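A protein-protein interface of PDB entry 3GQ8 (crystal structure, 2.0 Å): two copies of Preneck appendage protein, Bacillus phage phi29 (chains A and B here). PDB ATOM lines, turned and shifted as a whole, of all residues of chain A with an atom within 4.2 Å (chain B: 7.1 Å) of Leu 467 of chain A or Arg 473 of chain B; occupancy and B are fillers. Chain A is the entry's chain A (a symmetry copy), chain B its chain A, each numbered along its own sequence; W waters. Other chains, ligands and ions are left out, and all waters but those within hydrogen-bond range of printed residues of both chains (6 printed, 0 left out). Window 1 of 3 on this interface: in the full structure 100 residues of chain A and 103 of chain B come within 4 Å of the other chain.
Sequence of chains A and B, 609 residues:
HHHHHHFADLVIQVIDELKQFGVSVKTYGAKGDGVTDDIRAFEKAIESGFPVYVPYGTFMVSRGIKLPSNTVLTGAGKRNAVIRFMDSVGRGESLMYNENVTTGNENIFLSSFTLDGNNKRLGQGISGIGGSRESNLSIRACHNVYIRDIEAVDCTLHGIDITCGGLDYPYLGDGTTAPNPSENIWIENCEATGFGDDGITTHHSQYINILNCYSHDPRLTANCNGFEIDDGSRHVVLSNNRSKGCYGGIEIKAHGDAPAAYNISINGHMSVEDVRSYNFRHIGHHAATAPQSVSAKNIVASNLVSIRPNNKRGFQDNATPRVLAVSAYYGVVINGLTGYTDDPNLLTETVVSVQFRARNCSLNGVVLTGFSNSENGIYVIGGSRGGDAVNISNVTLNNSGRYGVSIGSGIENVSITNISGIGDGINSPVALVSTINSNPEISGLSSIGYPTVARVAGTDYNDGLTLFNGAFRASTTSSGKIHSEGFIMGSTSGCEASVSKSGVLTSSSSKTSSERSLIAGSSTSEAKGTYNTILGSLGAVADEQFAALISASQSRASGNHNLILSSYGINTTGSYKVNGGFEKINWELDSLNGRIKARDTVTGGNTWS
The backbone NH of Phe 468 of chain A lies within hydrogen-bond range of the backbone carbonyl oxygen of Arg 473 of chain B (3.0 Å).
The backbone NH (N) of Arg 473 of chain B sits at hydrogen-bond distance from the backbone carbonyl oxygen (O) of Thr 466 of chain A, at 3.1 Å.
The backbone NH of Thr 466 of chain A sits at hydrogen-bond distance from the backbone carbonyl oxygen of Ala 471 of chain B, at 2.8 Å.
OG of Ser 438 of chain A is in hydrogen-bond range of O of Thr 477 of chain B, 2.9 Å away.
NH2 of Arg 473 of chain B is in hydrogen-bond range of O of Ser 438 of chain A (2.9 Å).
The side-chain hydroxyl (OG1) of Thr 466 of chain A sits at hydrogen-bond distance from the backbone carbonyl oxygen (O) of Asn 469 of chain B (2.7 Å).
O of Ala 474 of chain B sits at hydrogen-bond distance from OG1 of Thr 476 of chain B.
O of Phe 472 of chain B is in hydrogen-bond range of N of Ile 488 of chain B, at 3.1 Å.
O of Ala 474 of chain B is in hydrogen-bond range of N of Gly 490 of chain B (3.2 Å).
O of Ile 442 of chain A lies within hydrogen-bond range of N of Leu 467 of chain A (2.8 Å).
The backbone NH (N) of Phe 472 of chain B sits at hydrogen-bond distance from the backbone carbonyl oxygen (O) of Gly 486 of chain B.
OG of Ser 475 of chain B sits at hydrogen-bond distance from N of Gly 490 of chain B, 3.0 Å away.
Among the printed residues, pairs that only touch across the chains: Asn 439 of chain A with Thr 477 of chain B (3.3 Å), Ser 438 of chain A with Ser 478 of chain B (3.4 Å), Thr 466 of chain A with Phe 472 of chain B (3.4 Å), Phe 468 of chain A with Ala 474 of chain B (3.5 Å), Leu 467 of chain A with Arg 473 of chain B (3.6 Å), Leu 465 of chain A with Ala 471 of chain B (3.6 Å), Thr 466 of chain A with Phe 468 of chain B (3.7 Å), Phe 468 of chain A with Ser 475 of chain B (3.7 Å), Phe 468 of chain A with Phe 468 of chain B (3.7 Å), Leu 465 of chain A with Asn 469 of chain B (3.8 Å), Asn 439 of chain A with Arg 473 of chain B (3.9 Å) and Leu 465 of chain A with Gly 470 of chain B (3.9 Å).
Of chain B, only Arg 473 (3.6 Å) comes within 4 Å of Leu 467 of chain A.
Arg 473 of chain B touches just these residues of chain A: Ser 438, Asn 439, Thr 466, Leu 467 and Phe 468.
Printed residues of chain B within 4 Å of Asn 439 of chain A: Arg 473 (3.9 Å) and Thr 477 (3.3 Å).
Printed residues of chain B within 4 Å of Ser 438 of chain A: Arg 473 (2.9 Å), Thr 477 (2.9 Å) and Ser 478 (3.4 Å).
Printed residues of chain A within 4 Å of Ser 475 of chain B: Phe 468 (3.7 Å).
Printed residues of chain A within 4 Å of Ala 471 of chain B: Leu 465 (3.6 Å) and Thr 466 (2.8 Å).
The nearest residue of chain B that does not touch Leu 467 of chain A is Ala 471 of chain B (5.1 Å).
The nearest printed residue of chain A that does not touch Arg 473 of chain B is Pro 440 of chain A (4.8 Å).
The nearest printed residue of chain A that does not touch Ser 475 of chain B is Leu 467 of chain A (7.2 Å).
Of the 9 printed residues of chain A, 6 touch a printed residue of chain B.
Printed residues of chain A that touch a printed residue of chain B: Ser 438, Asn 439, Leu 465, Thr 466, Leu 467 and Phe 468.
Among the printed residues, 18 pairs touch across the chains.
Phe 468 of chain B touches its own counterpart, Phe 468 of chain A.
Position printed for both chains: 468.
Of the 18 pairs that touch across the chains among the printed residues, 1 has its exchanged pair printed and touching as well.
Water W3 lies within hydrogen-bond range of O of Thr 476 of chain B (2.6 Å), O of Phe 468 of chain A (2.6 Å) and N of Ser 475 of chain B (3.3 Å).
Water W5 lies within hydrogen-bond range of the guanidinium group (NH1) of Arg 473 of chain B (2.7 Å), the backbone carbonyl oxygen (O) of Ser 438 of chain A (2.8 Å) and the backbone NH (N) of Ser 479 of chain B (3.4 Å).
Water W4 lies within hydrogen-bond range of the backbone carbonyl oxygen of Pro 440 of chain A (2.8 Å) and the guanidinium group of Arg 473 of chain B (2.9 Å).
Water W2 lies within hydrogen-bond range of O of Phe 468 of chain A (2.9 Å) and NE of Arg 473 of chain B (2.9 Å).
Water W1 bridges the backbone NH of Ser 475 of chain B (2.9 Å) and the backbone carbonyl oxygen of Phe 468 of chain A (3.2 Å).
Water W6 lies within hydrogen-bond range of OG1 of Thr 466 of chain A (2.9 Å), O of Leu 465 of chain A (3.1 Å) and O of Asn 469 of chain B (3.4 Å).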
ATOM      1  N   SER A 438      -5.982 -26.427 -11.938  1.00  0.00           N
ATOM      2  CA  SER A 438      -5.759 -25.231 -11.120  1.00  0.00           C
ATOM      3  C   SER A 438      -4.819 -25.439  -9.932  1.00  0.00           C
ATOM      4  O   SER A 438      -4.328 -24.455  -9.351  1.00  0.00           O
ATOM      5  CB  SER A 438      -7.101 -24.684 -10.626  1.00  0.00           C
ATOM      6  OG  SER A 438      -7.692 -25.617  -9.738  1.00  0.00           O
ATOM      7  N   ASN A 439      -4.568 -26.710  -9.589  1.00  0.00           N
ATOM      8  CA  ASN A 439      -3.836 -27.081  -8.373  1.00  0.00           C
ATOM      9  C   ASN A 439      -2.549 -27.905  -8.605  1.00  0.00           C
ATOM     10  O   ASN A 439      -2.352 -28.930  -7.939  1.00  0.00           O
ATOM     11  CB  ASN A 439      -4.759 -27.861  -7.433  1.00  0.00           C
ATOM     12  CG  ASN A 439      -5.205 -29.193  -8.037  1.00  0.00           C
ATOM     13  OD1 ASN A 439      -5.204 -29.354  -9.267  1.00  0.00           O
ATOM     14  ND2 ASN A 439      -5.547 -30.163  -7.178  1.00  0.00           N
ATOM     15  N   PRO A 440      -1.650 -27.446  -9.507  1.00  0.00           N
ATOM     16  CA  PRO A 440      -0.381 -28.152  -9.594  1.00  0.00           C
ATOM     17  C   PRO A 440       0.454 -27.824  -8.357  1.00  0.00           C
ATOM     18  O   PRO A 440       0.254 -26.770  -7.745  1.00  0.00           O
ATOM     19  CB  PRO A 440       0.266 -27.537 -10.834  1.00  0.00           C
ATOM     20  CG  PRO A 440      -0.260 -26.134 -10.871  1.00  0.00           C
ATOM     21  CD  PRO A 440      -1.687 -26.280 -10.414  1.00  0.00           C
ATOM     22  N   GLU A 441       1.348 -28.725  -7.954  1.00  0.00           N
ATOM     23  CA  GLU A 441       2.360 -28.343  -6.960  1.00  0.00           C
ATOM     24  C   GLU A 441       3.609 -27.873  -7.687  1.00  0.00           C
ATOM     25  O   GLU A 441       4.138 -28.572  -8.544  1.00  0.00           O
ATOM     26  CB  GLU A 441       2.660 -29.474  -5.959  1.00  0.00           C
ATOM     27  CG  GLU A 441       1.437 -29.780  -5.046  1.00  0.00           C
ATOM     28  CD  GLU A 441       1.773 -30.686  -3.872  1.00  0.00           C
ATOM     29  OE1 GLU A 441       2.206 -31.838  -4.123  1.00  0.00           O
ATOM     30  OE2 GLU A 441       1.608 -30.252  -2.703  1.00  0.00           O
ATOM     31  N   ILE A 442       4.065 -26.674  -7.354  1.00  0.00           N
ATOM     32  CA  ILE A 442       5.120 -26.018  -8.105  1.00  0.00           C
ATOM     33  C   ILE A 442       6.049 -25.265  -7.171  1.00  0.00           C
ATOM     34  O   ILE A 442       5.582 -24.577  -6.252  1.00  0.00           O
ATOM     35  CB  ILE A 442       4.544 -24.962  -9.092  1.00  0.00           C
ATOM     36  CG1 ILE A 442       3.730 -25.627 -10.205  1.00  0.00           C
ATOM     37  CG2 ILE A 442       5.684 -24.077  -9.667  1.00  0.00           C
ATOM     38  CD1 ILE A 442       3.088 -24.631 -11.210  1.00  0.00           C
ATOM     39  N   LEU A 465       6.954 -18.504  -7.779  1.00  0.00           N
ATOM     40  CA  LEU A 465       5.741 -19.175  -7.348  1.00  0.00           C
ATOM     41  C   LEU A 465       6.061 -20.378  -6.477  1.00  0.00           C
ATOM     42  O   LEU A 465       6.954 -21.156  -6.811  1.00  0.00           O
ATOM     43  CB  LEU A 465       4.976 -19.662  -8.588  1.00  0.00           C
ATOM     44  CG  LEU A 465       3.611 -20.299  -8.444  1.00  0.00           C
ATOM     45  CD1 LEU A 465       2.643 -19.337  -7.753  1.00  0.00           C
ATOM     46  CD2 LEU A 465       3.068 -20.697  -9.804  1.00  0.00           C
ATOM     47  N   THR A 466       5.308 -20.539  -5.387  1.00  0.00           N
ATOM     48  CA  THR A 466       5.336 -21.763  -4.580  1.00  0.00           C
ATOM     49  C   THR A 466       3.903 -22.198  -4.286  1.00  0.00           C
ATOM     50  O   THR A 466       3.174 -21.477  -3.596  1.00  0.00           O
ATOM     51  CB  THR A 466       6.072 -21.541  -3.234  1.00  0.00           C
ATOM     52  OG1 THR A 466       7.421 -21.146  -3.498  1.00  0.00           O
ATOM     53  CG2 THR A 466       6.078 -22.839  -2.397  1.00  0.00           C
ATOM     54  N   LEU A 467       3.497 -23.356  -4.808  1.00  0.00           N
ATOM     55  CA  LEU A 467       2.132 -23.857  -4.600  1.00  0.00           C
ATOM     56  C   LEU A 467       2.157 -25.238  -3.963  1.00  0.00           C
ATOM     57  O   LEU A 467       2.763 -26.149  -4.509  1.00  0.00           O
ATOM     58  CB  LEU A 467       1.358 -23.958  -5.933  1.00  0.00           C
ATOM     59  CG  LEU A 467       1.290 -22.749  -6.864  1.00  0.00           C
ATOM     60  CD1 LEU A 467       0.563 -23.121  -8.154  1.00  0.00           C
ATOM     61  CD2 LEU A 467       0.595 -21.593  -6.183  1.00  0.00           C
ATOM     62  N   PHE A 468       1.479 -25.397  -2.834  1.00  0.00           N
ATOM     63  CA  PHE A 468       1.350 -26.718  -2.213  1.00  0.00           C
ATOM     64  C   PHE A 468      -0.103 -27.101  -2.010  1.00  0.00           C
ATOM     65  O   PHE A 468      -0.953 -26.228  -1.859  1.00  0.00           O
ATOM     66  CB  PHE A 468       2.096 -26.760  -0.884  1.00  0.00           C
ATOM     67  CG  PHE A 468       3.587 -26.888  -1.044  1.00  0.00           C
ATOM     68  CD1 PHE A 468       4.406 -25.786  -0.889  1.00  0.00           C
ATOM     69  CD2 PHE A 468       4.160 -28.123  -1.368  1.00  0.00           C
ATOM     70  CE1 PHE A 468       5.781 -25.890  -1.044  1.00  0.00           C
ATOM     71  CE2 PHE A 468       5.539 -28.249  -1.522  1.00  0.00           C
ATOM     72  CZ  PHE A 468       6.352 -27.119  -1.361  1.00  0.00           C
ATOM     73  N   PHE B 468      10.684 -20.560   1.362  1.00  0.00           N
ATOM     74  CA  PHE B 468      10.236 -20.618  -0.032  1.00  0.00           C
ATOM     75  C   PHE B 468      10.100 -19.234  -0.633  1.00  0.00           C
ATOM     76  O   PHE B 468       9.851 -18.271   0.088  1.00  0.00           O
ATOM     77  CB  PHE B 468       8.914 -21.371  -0.137  1.00  0.00           C
ATOM     78  CG  PHE B 468       9.071 -22.864  -0.037  1.00  0.00           C
ATOM     79  CD1 PHE B 468       8.768 -23.523   1.139  1.00  0.00           C
ATOM     80  CD2 PHE B 468       9.541 -23.601  -1.130  1.00  0.00           C
ATOM     81  CE1 PHE B 468       8.919 -24.898   1.246  1.00  0.00           C
ATOM     82  CE2 PHE B 468       9.693 -24.983  -1.044  1.00  0.00           C
ATOM     83  CZ  PHE B 468       9.381 -25.632   0.158  1.00  0.00           C
ATOM     84  N   ASN B 469      10.259 -19.140  -1.952  1.00  0.00           N
ATOM     85  CA  ASN B 469      10.192 -17.850  -2.651  1.00  0.00           C
ATOM     86  C   ASN B 469       8.950 -17.683  -3.514  1.00  0.00           C
ATOM     87  O   ASN B 469       8.309 -18.679  -3.896  1.00  0.00           O
ATOM     88  CB  ASN B 469      11.422 -17.664  -3.544  1.00  0.00           C
ATOM     89  CG  ASN B 469      12.683 -17.419  -2.752  1.00  0.00           C
ATOM     90  OD1 ASN B 469      12.637 -17.045  -1.578  1.00  0.00           O
ATOM     91  ND2 ASN B 469      13.824 -17.634  -3.390  1.00  0.00           N
ATOM     92  N   GLY B 470       8.642 -16.423  -3.834  1.00  0.00           N
ATOM     93  CA  GLY B 470       7.573 -16.064  -4.752  1.00  0.00           C
ATOM     94  C   GLY B 470       6.187 -16.092  -4.143  1.00  0.00           C
ATOM     95  O   GLY B 470       6.029 -16.366  -2.957  1.00  0.00           O
ATOM     96  N   ALA B 471       5.177 -15.806  -4.961  1.00  0.00           N
ATOM     97  CA  ALA B 471       3.784 -15.925  -4.550  1.00  0.00           C
ATOM     98  C   ALA B 471       3.584 -17.260  -3.837  1.00  0.00           C
ATOM     99  O   ALA B 471       4.101 -18.285  -4.289  1.00  0.00           O
ATOM    100  CB  ALA B 471       2.878 -15.833  -5.763  1.00  0.00           C
ATOM    101  N   PHE B 472       2.849 -17.258  -2.728  1.00  0.00           N
ATOM    102  CA  PHE B 472       2.682 -18.495  -1.950  1.00  0.00           C
ATOM    103  C   PHE B 472       1.222 -18.888  -1.814  1.00  0.00           C
ATOM    104  O   PHE B 472       0.388 -18.036  -1.509  1.00  0.00           O
ATOM    105  CB  PHE B 472       3.297 -18.360  -0.544  1.00  0.00           C
ATOM    106  CG  PHE B 472       3.178 -19.618   0.283  1.00  0.00           C
ATOM    107  CD1 PHE B 472       3.974 -20.722   0.006  1.00  0.00           C
ATOM    108  CD2 PHE B 472       2.247 -19.709   1.317  1.00  0.00           C
ATOM    109  CE1 PHE B 472       3.859 -21.902   0.753  1.00  0.00           C
ATOM    110  CE2 PHE B 472       2.131 -20.894   2.083  1.00  0.00           C
ATOM    111  CZ  PHE B 472       2.941 -21.987   1.788  1.00  0.00           C
ATOM    112  N   ARG B 473       0.910 -20.169  -2.020  1.00  0.00           N
ATOM    113  CA  ARG B 473      -0.457 -20.664  -1.815  1.00  0.00           C
ATOM    114  C   ARG B 473      -0.433 -22.061  -1.224  1.00  0.00           C
ATOM    115  O   ARG B 473       0.319 -22.927  -1.683  1.00  0.00           O
ATOM    116  CB  ARG B 473      -1.272 -20.664  -3.123  1.00  0.00           C
ATOM    117  CG  ARG B 473      -2.792 -20.856  -2.906  1.00  0.00           C
ATOM    118  CD  ARG B 473      -3.564 -20.911  -4.234  1.00  0.00           C
ATOM    119  NE  ARG B 473      -3.236 -22.127  -4.976  1.00  0.00           N
ATOM    120  CZ  ARG B 473      -3.616 -22.386  -6.223  1.00  0.00           C
ATOM    121  NH1 ARG B 473      -4.335 -21.501  -6.919  1.00  0.00           N
ATOM    122  NH2 ARG B 473      -3.268 -23.532  -6.778  1.00  0.00           N
ATOM    123  N   ALA B 474      -1.248 -22.277  -0.196  1.00  0.00           N
ATOM    124  CA  ALA B 474      -1.387 -23.603   0.395  1.00  0.00           C
ATOM    125  C   ALA B 474      -2.827 -23.849   0.779  1.00  0.00           C
ATOM    126  O   ALA B 474      -3.584 -22.899   1.006  1.00  0.00           O
ATOM    127  CB  ALA B 474      -0.482 -23.752   1.630  1.00  0.00           C
ATOM    128  N   SER B 475      -3.182 -25.134   0.873  1.00  0.00           N
ATOM    129  CA  SER B 475      -4.518 -25.599   1.258  1.00  0.00           C
ATOM    130  C   SER B 475      -5.647 -24.826   0.572  1.00  0.00           C
ATOM    131  O   SER B 475      -6.657 -24.505   1.203  1.00  0.00           O
ATOM    132  CB  SER B 475      -4.692 -25.632   2.790  1.00  0.00           C
ATOM    133  OG  SER B 475      -4.353 -24.398   3.422  1.00  0.00           O
ATOM    134  N   THR B 476      -5.458 -24.561  -0.725  1.00  0.00           N
ATOM    135  CA  THR B 476      -6.391 -23.796  -1.560  1.00  0.00           C
ATOM    136  C   THR B 476      -6.294 -24.402  -2.962  1.00  0.00           C
ATOM    137  O   THR B 476      -5.245 -24.328  -3.596  1.00  0.00           O
ATOM    138  CB  THR B 476      -6.007 -22.279  -1.597  1.00  0.00           C
ATOM    139  OG1 THR B 476      -5.901 -21.775  -0.259  1.00  0.00           O
ATOM    140  CG2 THR B 476      -7.049 -21.435  -2.358  1.00  0.00           C
ATOM    141  N   THR B 477      -7.374 -24.996  -3.454  1.00  0.00           N
ATOM    142  CA  THR B 477      -7.321 -25.739  -4.726  1.00  0.00           C
ATOM    143  C   THR B 477      -7.322 -24.864  -5.991  1.00  0.00           C
ATOM    144  O   THR B 477      -6.816 -25.292  -7.029  1.00  0.00           O
ATOM    145  CB  THR B 477      -8.450 -26.800  -4.823  1.00  0.00           C
ATOM    146  OG1 THR B 477      -9.716 -26.139  -4.766  1.00  0.00           O
ATOM    147  CG2 THR B 477      -8.369 -27.781  -3.673  1.00  0.00           C
ATOM    148  N   SER B 478      -7.903 -23.667  -5.919  1.00  0.00           N
ATOM    149  CA  SER B 478      -7.789 -22.675  -7.003  1.00  0.00           C
ATOM    150  C   SER B 478      -7.896 -21.255  -6.471  1.00  0.00           C
ATOM    151  O   SER B 478      -8.453 -21.027  -5.392  1.00  0.00           O
ATOM    152  CB  SER B 478      -8.844 -22.874  -8.103  1.00  0.00           C
ATOM    153  OG  SER B 478     -10.136 -22.645  -7.596  1.00  0.00           O
ATOM    154  N   SER B 479      -7.363 -20.311  -7.241  1.00  0.00           N
ATOM    155  CA  SER B 479      -7.406 -18.906  -6.879  1.00  0.00           C
ATOM    156  C   SER B 479      -7.121 -18.068  -8.111  1.00  0.00           C
ATOM    157  O   SER B 479      -6.673 -18.586  -9.139  1.00  0.00           O
ATOM    158  CB  SER B 479      -6.371 -18.583  -5.789  1.00  0.00           C
ATOM    159  OG  SER B 479      -5.068 -18.579  -6.334  1.00  0.00           O
ATOM    160  N   GLY B 480      -7.391 -16.777  -7.990  1.00  0.00           N
ATOM    161  CA  GLY B 480      -6.923 -15.792  -8.949  1.00  0.00           C
ATOM    162  C   GLY B 480      -5.485 -15.425  -8.616  1.00  0.00           C
ATOM    163  O   GLY B 480      -4.743 -16.218  -8.011  1.00  0.00           O
ATOM    164  N   ILE B 482      -1.932 -14.077  -7.263  1.00  0.00           N
ATOM    165  CA  ILE B 482      -1.214 -13.847  -6.013  1.00  0.00           C
ATOM    166  C   ILE B 482       0.105 -13.146  -6.328  1.00  0.00           C
ATOM    167  O   ILE B 482       0.889 -13.639  -7.129  1.00  0.00           O
ATOM    168  CB  ILE B 482      -0.932 -15.167  -5.250  1.00  0.00           C
ATOM    169  CG1 ILE B 482      -2.226 -15.964  -5.067  1.00  0.00           C
ATOM    170  CG2 ILE B 482      -0.288 -14.876  -3.892  1.00  0.00           C
ATOM    171  CD1 ILE B 482      -2.028 -17.340  -4.460  1.00  0.00           C
ATOM    172  N   GLY B 486       2.831 -11.867  -1.591  1.00  0.00           N
ATOM    173  CA  GLY B 486       1.466 -12.120  -1.147  1.00  0.00           C
ATOM    174  C   GLY B 486       1.241 -13.609  -0.917  1.00  0.00           C
ATOM    175  O   GLY B 486       2.118 -14.429  -1.224  1.00  0.00           O
ATOM    176  N   PHE B 487       0.062 -13.959  -0.403  1.00  0.00           N
ATOM    177  CA  PHE B 487      -0.286 -15.359  -0.127  1.00  0.00           C
ATOM    178  C   PHE B 487      -1.788 -15.550  -0.065  1.00  0.00           C
ATOM    179  O   PHE B 487      -2.534 -14.602   0.206  1.00  0.00           O
ATOM    180  CB  PHE B 487       0.340 -15.871   1.198  1.00  0.00           C
ATOM    181  CG  PHE B 487      -0.068 -15.081   2.408  1.00  0.00           C
ATOM    182  CD1 PHE B 487       0.770 -14.081   2.905  1.00  0.00           C
ATOM    183  CD2 PHE B 487      -1.291 -15.321   3.051  1.00  0.00           C
ATOM    184  CE1 PHE B 487       0.402 -13.337   4.012  1.00  0.00           C
ATOM    185  CE2 PHE B 487      -1.680 -14.556   4.163  1.00  0.00           C
ATOM    186  CZ  PHE B 487      -0.831 -13.568   4.640  1.00  0.00           C
ATOM    187  N   ILE B 488      -2.212 -16.781  -0.332  1.00  0.00           N
ATOM    188  CA  ILE B 488      -3.567 -17.237  -0.021  1.00  0.00           C
ATOM    189  C   ILE B 488      -3.437 -18.606   0.650  1.00  0.00           C
ATOM    190  O   ILE B 488      -2.720 -19.481   0.145  1.00  0.00           O
ATOM    191  CB  ILE B 488      -4.460 -17.357  -1.278  1.00  0.00           C
ATOM    192  CG1 ILE B 488      -4.591 -15.991  -1.987  1.00  0.00           C
ATOM    193  CG2 ILE B 488      -5.871 -17.914  -0.898  1.00  0.00           C
ATOM    194  CD1 ILE B 488      -5.337 -16.030  -3.325  1.00  0.00           C
ATOM    195  N   MET B 489      -4.108 -18.790   1.785  1.00  0.00           N
ATOM    196  CA  MET B 489      -4.117 -20.091   2.458  1.00  0.00           C
ATOM    197  C   MET B 489      -5.485 -20.486   3.002  1.00  0.00           C
ATOM    198  O   MET B 489      -6.263 -19.619   3.403  1.00  0.00           O
ATOM    199  CB  MET B 489      -3.117 -20.114   3.613  1.00  0.00           C
ATOM    200  CG  MET B 489      -1.662 -19.900   3.211  1.00  0.00           C
ATOM    201  SD  MET B 489      -0.609 -20.109   4.681  1.00  0.00           S
ATOM    202  CE  MET B 489      -1.087 -21.716   5.232  1.00  0.00           C
ATOM    203  N   GLY B 490      -5.743 -21.801   3.028  1.00  0.00           N
ATOM    204  CA  GLY B 490      -6.948 -22.378   3.642  1.00  0.00           C
ATOM    205  C   GLY B 490      -8.212 -21.754   3.112  1.00  0.00           C
ATOM    206  O   GLY B 490      -9.135 -21.467   3.867  1.00  0.00           O
HETATM  207  O   HOH W   1      -1.137 -27.120   1.248  1.00  0.00           O
HETATM  208  O   HOH W   2      -1.628 -24.254  -3.819  1.00  0.00           O
HETATM  209  O   HOH W   3      -3.440 -25.673  -2.328  1.00  0.00           O
HETATM  210  O   HOH W   4      -1.842 -25.945  -6.041  1.00  0.00           O
HETATM  211  O   HOH W   5      -5.345 -21.885  -9.425  1.00  0.00           O
HETATM  212  O   HOH W   6       9.674 -21.399  -5.379  1.00  0.00           O
